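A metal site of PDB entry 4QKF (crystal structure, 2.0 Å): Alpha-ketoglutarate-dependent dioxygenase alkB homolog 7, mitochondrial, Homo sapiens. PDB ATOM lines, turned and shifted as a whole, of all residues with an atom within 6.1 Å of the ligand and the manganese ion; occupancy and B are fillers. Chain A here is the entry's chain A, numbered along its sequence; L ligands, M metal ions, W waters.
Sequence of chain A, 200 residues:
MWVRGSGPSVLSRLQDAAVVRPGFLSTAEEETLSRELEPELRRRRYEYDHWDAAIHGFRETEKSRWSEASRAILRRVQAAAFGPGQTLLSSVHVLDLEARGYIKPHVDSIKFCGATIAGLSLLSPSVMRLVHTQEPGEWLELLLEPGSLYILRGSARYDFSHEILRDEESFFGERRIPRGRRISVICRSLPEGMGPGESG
OD1 of Asp 108 is bound to the manganese ion, at 2.3 Å. The manganese ion is bound by NE2 of His 106. A ring nitrogen (NE2) of His 162 is bound to the manganese ion (2.4 Å). O3 of the ligand is bound to the manganese ion. Slightly farther from the manganese ion lies O2 of the ligand (2.7 Å).
The backbone carbonyl oxygen (O) of Leu 95 sits at hydrogen-bond distance from the backbone NH (N) of Ser 184 (2.7 Å). A ring nitrogen (ND1) of His 93 sits at hydrogen-bond distance from the guanidinium group (NH1) of Arg 188 (2.9 Å). The backbone NH (N) of Tyr 150 sits at hydrogen-bond distance from the backbone carbonyl oxygen (O) of Gly 119, 2.9 Å away. The side-chain carboxylate of Asp 108 lies within salt-bridge range of the guanidinium group of Arg 188, 2.7 Å away. O of Ile 164 sits at hydrogen-bond distance from N of Ile 103 (3.0 Å). O of His 93 lies within hydrogen-bond range of N of Ile 186, at 2.8 Å. O of Arg 182 is in hydrogen-bond range of N of Leu 97. OG of Ser 184 is in hydrogen-bond range of NH1 of Arg 182.
Three residues have an atom within 4 Å of the manganese ion: His 106, Asp 108 and His 162. The nearest printed residue that does not touch the manganese ion is Arg 188 (4.2 Å).
An oxygen (O4) of the ligand sits at hydrogen-bond distance from the side-chain hydroxyl (OG) of Ser 184 (2.6 Å). An oxygen (O5) of the ligand sits at hydrogen-bond distance from the side-chain hydroxyl of Tyr 150, at 2.6 Å. The guanidinium group (NH1) of Arg 182 lies within salt-bridge range of an oxygen (O4) of the ligand. The guanidinium group of Arg 188 lies within salt-bridge range of an oxygen (O1) of the ligand.
His 93 touches the ligand. CD2 of Leu 95 touches O4 of the ligand, at 3.7 Å. Ile 164 touches the ligand (CD1 to C3, 3.5 Å). Ile 186 touches the ligand (CD1 to N1, 3.8 Å). Hydrophobic or aromatic side chains that line the ligand: His 93, Leu 95, His 106, Tyr 150, His 162, Ile 164 and Ile 186. The nearest printed residue that does not touch the ligand is Ile 103 (4.1 Å).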
ATOM      1  N   ALA A  54      -5.399 -14.975  19.243  1.00  0.00           N
ATOM      2  CA  ALA A  54      -4.641 -15.402  18.060  1.00  0.00           C
ATOM      3  C   ALA A  54      -4.248 -16.892  18.134  1.00  0.00           C
ATOM      4  O   ALA A  54      -4.351 -17.606  17.160  1.00  0.00           O
ATOM      5  CB  ALA A  54      -3.400 -14.540  17.925  1.00  0.00           C
ATOM      6  N   ILE A  55      -3.866 -17.342  19.316  1.00  0.00           N
ATOM      7  CA  ILE A  55      -3.351 -18.694  19.520  1.00  0.00           C
ATOM      8  C   ILE A  55      -4.413 -19.524  20.204  1.00  0.00           C
ATOM      9  O   ILE A  55      -4.972 -19.088  21.233  1.00  0.00           O
ATOM     10  CB  ILE A  55      -2.097 -18.669  20.401  1.00  0.00           C
ATOM     11  CG1 ILE A  55      -1.186 -17.521  20.010  1.00  0.00           C
ATOM     12  CG2 ILE A  55      -1.347 -19.995  20.346  1.00  0.00           C
ATOM     13  CD1 ILE A  55      -0.147 -17.206  21.066  1.00  0.00           C
ATOM     14  N   HIS A  93      10.243 -16.199  24.041  1.00  0.00           N
ATOM     15  CA  HIS A  93       8.900 -16.740  24.077  1.00  0.00           C
ATOM     16  C   HIS A  93       8.838 -18.187  23.557  1.00  0.00           C
ATOM     17  O   HIS A  93       9.145 -18.488  22.384  1.00  0.00           O
ATOM     18  CB  HIS A  93       7.966 -15.780  23.314  1.00  0.00           C
ATOM     19  CG  HIS A  93       6.632 -16.355  23.026  1.00  0.00           C
ATOM     20  ND1 HIS A  93       5.931 -16.083  21.865  1.00  0.00           N
ATOM     21  CD2 HIS A  93       5.848 -17.188  23.746  1.00  0.00           C
ATOM     22  CE1 HIS A  93       4.800 -16.742  21.873  1.00  0.00           C
ATOM     23  NE2 HIS A  93       4.722 -17.417  23.003  1.00  0.00           N
ATOM     24  N   LEU A  95       6.538 -21.288  22.812  1.00  0.00           N
ATOM     25  CA  LEU A  95       5.170 -21.602  22.548  1.00  0.00           C
ATOM     26  C   LEU A  95       4.928 -23.070  22.183  1.00  0.00           C
ATOM     27  O   LEU A  95       5.446 -23.556  21.162  1.00  0.00           O
ATOM     28  CB  LEU A  95       4.708 -20.716  21.395  1.00  0.00           C
ATOM     29  CG  LEU A  95       3.275 -20.862  20.979  1.00  0.00           C
ATOM     30  CD1 LEU A  95       2.333 -20.641  22.156  1.00  0.00           C
ATOM     31  CD2 LEU A  95       2.988 -19.862  19.865  1.00  0.00           C
ATOM     32  N   LEU A  97       2.330 -25.692  20.914  1.00  0.00           N
ATOM     33  CA  LEU A  97       1.026 -25.950  20.302  1.00  0.00           C
ATOM     34  C   LEU A  97       0.718 -27.432  20.318  1.00  0.00           C
ATOM     35  O   LEU A  97       1.555 -28.280  19.980  1.00  0.00           O
ATOM     36  CB  LEU A  97       0.922 -25.426  18.866  1.00  0.00           C
ATOM     37  CG  LEU A  97       0.712 -23.922  18.614  1.00  0.00           C
ATOM     38  CD1 LEU A  97       0.449 -23.696  17.142  1.00  0.00           C
ATOM     39  CD2 LEU A  97      -0.402 -23.268  19.462  1.00  0.00           C
ATOM     40  N   ILE A 103      -2.665 -21.193  15.100  1.00  0.00           N
ATOM     41  CA  ILE A 103      -2.485 -19.766  15.258  1.00  0.00           C
ATOM     42  C   ILE A 103      -3.175 -19.026  14.124  1.00  0.00           C
ATOM     43  O   ILE A 103      -2.968 -19.312  12.930  1.00  0.00           O
ATOM     44  CB  ILE A 103      -0.993 -19.403  15.341  1.00  0.00           C
ATOM     45  CG1 ILE A 103      -0.318 -20.261  16.403  1.00  0.00           C
ATOM     46  CG2 ILE A 103      -0.837 -17.929  15.628  1.00  0.00           C
ATOM     47  CD1 ILE A 103       1.042 -19.797  16.881  1.00  0.00           C
ATOM     48  N   HIS A 106      -2.192 -12.834  12.298  1.00  0.00           N
ATOM     49  CA  HIS A 106      -1.954 -11.617  13.058  1.00  0.00           C
ATOM     50  C   HIS A 106      -0.627 -11.024  12.765  1.00  0.00           C
ATOM     51  O   HIS A 106       0.286 -11.669  12.258  1.00  0.00           O
ATOM     52  CB  HIS A 106      -1.952 -11.924  14.534  1.00  0.00           C
ATOM     53  CG  HIS A 106      -0.966 -12.983  14.882  1.00  0.00           C
ATOM     54  ND1 HIS A 106      -1.098 -14.279  14.446  1.00  0.00           N
ATOM     55  CD2 HIS A 106       0.184 -12.925  15.581  1.00  0.00           C
ATOM     56  CE1 HIS A 106      -0.077 -14.992  14.878  1.00  0.00           C
ATOM     57  NE2 HIS A 106       0.738 -14.188  15.538  1.00  0.00           N
ATOM     58  N   VAL A 107      -0.483  -9.781  13.170  1.00  0.00           N
ATOM     59  CA  VAL A 107       0.800  -9.155  13.159  1.00  0.00           C
ATOM     60  C   VAL A 107       1.200  -9.012  14.613  1.00  0.00           C
ATOM     61  O   VAL A 107       0.362  -8.700  15.448  1.00  0.00           O
ATOM     62  CB  VAL A 107       0.697  -7.810  12.432  1.00  0.00           C
ATOM     63  CG1 VAL A 107       1.973  -7.026  12.599  1.00  0.00           C
ATOM     64  CG2 VAL A 107       0.392  -8.067  10.949  1.00  0.00           C
ATOM     65  N   ASP A 108       2.487  -9.165  14.900  1.00  0.00           N
ATOM     66  CA  ASP A 108       2.999  -9.016  16.232  1.00  0.00           C
ATOM     67  C   ASP A 108       2.990  -7.574  16.662  1.00  0.00           C
ATOM     68  O   ASP A 108       3.358  -6.700  15.884  1.00  0.00           O
ATOM     69  CB  ASP A 108       4.441  -9.482  16.337  1.00  0.00           C
ATOM     70  CG  ASP A 108       4.544 -10.941  16.559  1.00  0.00           C
ATOM     71  OD1 ASP A 108       3.626 -11.639  16.146  1.00  0.00           O
ATOM     72  OD2 ASP A 108       5.538 -11.411  17.114  1.00  0.00           O
ATOM     73  N   ILE A 117      11.332 -10.852  13.766  1.00  0.00           N
ATOM     74  CA  ILE A 117      10.863 -12.021  14.491  1.00  0.00           C
ATOM     75  C   ILE A 117      11.594 -13.256  13.938  1.00  0.00           C
ATOM     76  O   ILE A 117      11.640 -13.463  12.724  1.00  0.00           O
ATOM     77  CB  ILE A 117       9.358 -12.192  14.308  1.00  0.00           C
ATOM     78  CG1 ILE A 117       8.585 -11.014  14.935  1.00  0.00           C
ATOM     79  CG2 ILE A 117       8.904 -13.493  14.930  1.00  0.00           C
ATOM     80  CD1 ILE A 117       7.284 -10.744  14.285  1.00  0.00           C
ATOM     81  N   GLY A 119      11.678 -17.488  14.571  1.00  0.00           N
ATOM     82  CA  GLY A 119      11.248 -18.680  15.267  1.00  0.00           C
ATOM     83  C   GLY A 119      11.997 -19.951  14.899  1.00  0.00           C
ATOM     84  O   GLY A 119      12.183 -20.246  13.710  1.00  0.00           O
ATOM     85  N   LEU A 120      12.406 -20.708  15.930  1.00  0.00           N
ATOM     86  CA  LEU A 120      12.796 -22.114  15.767  1.00  0.00           C
ATOM     87  C   LEU A 120      11.619 -23.026  15.902  1.00  0.00           C
ATOM     88  O   LEU A 120      10.704 -22.776  16.703  1.00  0.00           O
ATOM     89  CB  LEU A 120      13.892 -22.484  16.789  1.00  0.00           C
ATOM     90  CG  LEU A 120      15.136 -21.644  16.644  1.00  0.00           C
ATOM     91  CD1 LEU A 120      16.106 -21.779  17.818  1.00  0.00           C
ATOM     92  CD2 LEU A 120      15.839 -22.013  15.348  1.00  0.00           C
ATOM     93  N   MET A 128       3.441 -21.992   7.962  1.00  0.00           N
ATOM     94  CA  MET A 128       3.063 -20.606   8.311  1.00  0.00           C
ATOM     95  C   MET A 128       2.621 -19.824   7.055  1.00  0.00           C
ATOM     96  O   MET A 128       3.368 -19.738   6.072  1.00  0.00           O
ATOM     97  CB  MET A 128       4.248 -19.925   8.940  1.00  0.00           C
ATOM     98  CG  MET A 128       4.187 -18.414   8.954  1.00  0.00           C
ATOM     99  SD  MET A 128       5.608 -17.803   9.803  1.00  0.00           S
ATOM    100  CE  MET A 128       5.371 -18.473  11.446  1.00  0.00           C
ATOM    101  N   TYR A 150      12.819 -19.752  10.936  1.00  0.00           N
ATOM    102  CA  TYR A 150      12.295 -18.690  10.045  1.00  0.00           C
ATOM    103  C   TYR A 150      12.662 -17.339  10.615  1.00  0.00           C
ATOM    104  O   TYR A 150      12.911 -17.204  11.832  1.00  0.00           O
ATOM    105  CB  TYR A 150      10.797 -18.796   9.770  1.00  0.00           C
ATOM    106  CG  TYR A 150       9.898 -18.519  10.946  1.00  0.00           C
ATOM    107  CD1 TYR A 150       9.534 -17.223  11.299  1.00  0.00           C
ATOM    108  CD2 TYR A 150       9.412 -19.563  11.738  1.00  0.00           C
ATOM    109  CE1 TYR A 150       8.709 -16.969  12.385  1.00  0.00           C
ATOM    110  CE2 TYR A 150       8.579 -19.321  12.840  1.00  0.00           C
ATOM    111  CZ  TYR A 150       8.234 -18.022  13.150  1.00  0.00           C
ATOM    112  OH  TYR A 150       7.407 -17.752  14.253  1.00  0.00           O
ATOM    113  N   HIS A 162       0.587 -13.292   9.737  1.00  0.00           N
ATOM    114  CA  HIS A 162       1.111 -14.605   9.669  1.00  0.00           C
ATOM    115  C   HIS A 162       0.424 -15.516  10.686  1.00  0.00           C
ATOM    116  O   HIS A 162      -0.043 -15.063  11.756  1.00  0.00           O
ATOM    117  CB  HIS A 162       2.602 -14.541   9.883  1.00  0.00           C
ATOM    118  CG  HIS A 162       2.986 -14.177  11.271  1.00  0.00           C
ATOM    119  ND1 HIS A 162       3.622 -13.003  11.592  1.00  0.00           N
ATOM    120  CD2 HIS A 162       2.821 -14.855  12.434  1.00  0.00           C
ATOM    121  CE1 HIS A 162       3.853 -12.981  12.893  1.00  0.00           C
ATOM    122  NE2 HIS A 162       3.396 -14.099  13.419  1.00  0.00           N
ATOM    123  N   GLU A 163       0.344 -16.780  10.327  1.00  0.00           N
ATOM    124  CA  GLU A 163      -0.481 -17.771  11.024  1.00  0.00           C
ATOM    125  C   GLU A 163       0.132 -19.152  10.842  1.00  0.00           C
ATOM    126  O   GLU A 163       0.829 -19.388   9.847  1.00  0.00           O
ATOM    127  CB  GLU A 163      -1.884 -17.754  10.457  1.00  0.00           C
ATOM    128  CG  GLU A 163      -1.971 -18.218   9.025  1.00  0.00           C
ATOM    129  CD  GLU A 163      -3.252 -17.836   8.362  1.00  0.00           C
ATOM    130  OE1 GLU A 163      -4.255 -18.569   8.489  1.00  0.00           O
ATOM    131  OE2 GLU A 163      -3.237 -16.779   7.696  1.00  0.00           O
ATOM    132  N   ILE A 164      -0.119 -20.062  11.782  1.00  0.00           N
ATOM    133  CA  ILE A 164       0.295 -21.459  11.658  1.00  0.00           C
ATOM    134  C   ILE A 164      -0.961 -22.262  11.499  1.00  0.00           C
ATOM    135  O   ILE A 164      -1.827 -22.249  12.377  1.00  0.00           O
ATOM    136  CB  ILE A 164       1.083 -21.975  12.884  1.00  0.00           C
ATOM    137  CG1 ILE A 164       2.454 -21.318  12.961  1.00  0.00           C
ATOM    138  CG2 ILE A 164       1.291 -23.481  12.790  1.00  0.00           C
ATOM    139  CD1 ILE A 164       2.464 -19.912  13.544  1.00  0.00           C
ATOM    140  N   ARG A 182       3.830 -29.146  18.475  1.00  0.00           N
ATOM    141  CA  ARG A 182       4.973 -28.423  17.951  1.00  0.00           C
ATOM    142  C   ARG A 182       5.320 -27.349  18.948  1.00  0.00           C
ATOM    143  O   ARG A 182       4.477 -26.551  19.336  1.00  0.00           O
ATOM    144  CB  ARG A 182       4.632 -27.740  16.606  1.00  0.00           C
ATOM    145  CG  ARG A 182       5.450 -26.480  16.317  1.00  0.00           C
ATOM    146  CD  ARG A 182       4.837 -25.634  15.191  1.00  0.00           C
ATOM    147  NE  ARG A 182       5.800 -24.662  14.674  1.00  0.00           N
ATOM    148  CZ  ARG A 182       5.889 -23.384  15.017  1.00  0.00           C
ATOM    149  NH1 ARG A 182       5.059 -22.843  15.927  1.00  0.00           N
ATOM    150  NH2 ARG A 182       6.850 -22.635  14.475  1.00  0.00           N
ATOM    151  N   ILE A 183       6.572 -27.316  19.342  1.00  0.00           N
ATOM    152  CA  ILE A 183       7.049 -26.246  20.175  1.00  0.00           C
ATOM    153  C   ILE A 183       7.757 -25.220  19.286  1.00  0.00           C
ATOM    154  O   ILE A 183       8.463 -25.603  18.351  1.00  0.00           O
ATOM    155  CB  ILE A 183       7.953 -26.757  21.293  1.00  0.00           C
ATOM    156  CG1 ILE A 183       7.220 -27.828  22.134  1.00  0.00           C
ATOM    157  CG2 ILE A 183       8.379 -25.620  22.191  1.00  0.00           C
ATOM    158  CD1 ILE A 183       8.111 -28.565  23.120  1.00  0.00           C
ATOM    159  N   SER A 184       7.542 -23.948  19.586  1.00  0.00           N
ATOM    160  CA  SER A 184       8.262 -22.842  18.951  1.00  0.00           C
ATOM    161  C   SER A 184       9.079 -22.138  19.994  1.00  0.00           C
ATOM    162  O   SER A 184       8.628 -21.908  21.130  1.00  0.00           O
ATOM    163  CB  SER A 184       7.304 -21.814  18.341  1.00  0.00           C
ATOM    164  OG  SER A 184       5.941 -22.187  18.508  1.00  0.00           O
ATOM    165  N   VAL A 185      10.286 -21.771  19.607  1.00  0.00           N
ATOM    166  CA  VAL A 185      11.125 -20.932  20.425  1.00  0.00           C
ATOM    167  C   VAL A 185      11.320 -19.659  19.642  1.00  0.00           C
ATOM    168  O   VAL A 185      11.979 -19.675  18.580  1.00  0.00           O
ATOM    169  CB  VAL A 185      12.471 -21.603  20.668  1.00  0.00           C
ATOM    170  CG1 VAL A 185      13.368 -20.734  21.515  1.00  0.00           C
ATOM    171  CG2 VAL A 185      12.247 -22.969  21.319  1.00  0.00           C
ATOM    172  N   ILE A 186      10.734 -18.570  20.140  1.00  0.00           N
ATOM    173  CA  ILE A 186      10.740 -17.314  19.381  1.00  0.00           C
ATOM    174  C   ILE A 186      11.562 -16.193  20.020  1.00  0.00           C
ATOM    175  O   ILE A 186      11.466 -15.903  21.225  1.00  0.00           O
ATOM    176  CB  ILE A 186       9.308 -16.855  19.073  1.00  0.00           C
ATOM    177  CG1 ILE A 186       9.297 -15.565  18.233  1.00  0.00           C
ATOM    178  CG2 ILE A 186       8.519 -16.589  20.334  1.00  0.00           C
ATOM    179  CD1 ILE A 186       8.125 -15.578  17.300  1.00  0.00           C
ATOM    180  N   ARG A 188      12.660 -12.143  19.770  1.00  0.00           N
ATOM    181  CA  ARG A 188      12.133 -10.905  19.197  1.00  0.00           C
ATOM    182  C   ARG A 188      13.043  -9.732  19.466  1.00  0.00           C
ATOM    183  O   ARG A 188      13.840  -9.746  20.383  1.00  0.00           O
ATOM    184  CB  ARG A 188      10.685 -10.665  19.667  1.00  0.00           C
ATOM    185  CG  ARG A 188       9.622 -11.517  19.033  1.00  0.00           C
ATOM    186  CD  ARG A 188       8.286 -11.275  19.722  1.00  0.00           C
ATOM    187  NE  ARG A 188       7.175 -12.002  19.156  1.00  0.00           N
ATOM    188  CZ  ARG A 188       6.643 -13.118  19.645  1.00  0.00           C
ATOM    189  NH1 ARG A 188       7.138 -13.699  20.731  1.00  0.00           N
ATOM    190  NH2 ARG A 188       5.628 -13.669  19.028  1.00  0.00           N
HETATM  191  C1  LIG L   1       3.144 -15.832  17.814  1.00  0.00           C
HETATM  192  C2  LIG L   1       3.641 -16.338  16.532  1.00  0.00           C
HETATM  193  C3  LIG L   1       4.773 -18.284  15.692  1.00  0.00           C
HETATM  194  C4  LIG L   1       5.660 -19.341  16.335  1.00  0.00           C
HETATM  195  O1  LIG L   1       3.792 -15.967  18.847  1.00  0.00           O
HETATM  196  O2  LIG L   1       2.053 -15.264  17.872  1.00  0.00           O
HETATM  197  O3  LIG L   1       2.906 -16.213  15.568  1.00  0.00           O
HETATM  198  O4  LIG L   1       5.091 -20.354  16.807  1.00  0.00           O
HETATM  199  N1  LIG L   1       4.746 -17.090  16.506  1.00  0.00           N
HETATM  200  O5  LIG L   1       6.905 -19.148  16.426  1.00  0.00           O
HETATM  201 MN    MN M   1       3.072 -13.836  15.755  1.00  0.00          MN
HETATM  202  O   HOH W   1       1.277 -12.884  18.464  1.00  0.00           O
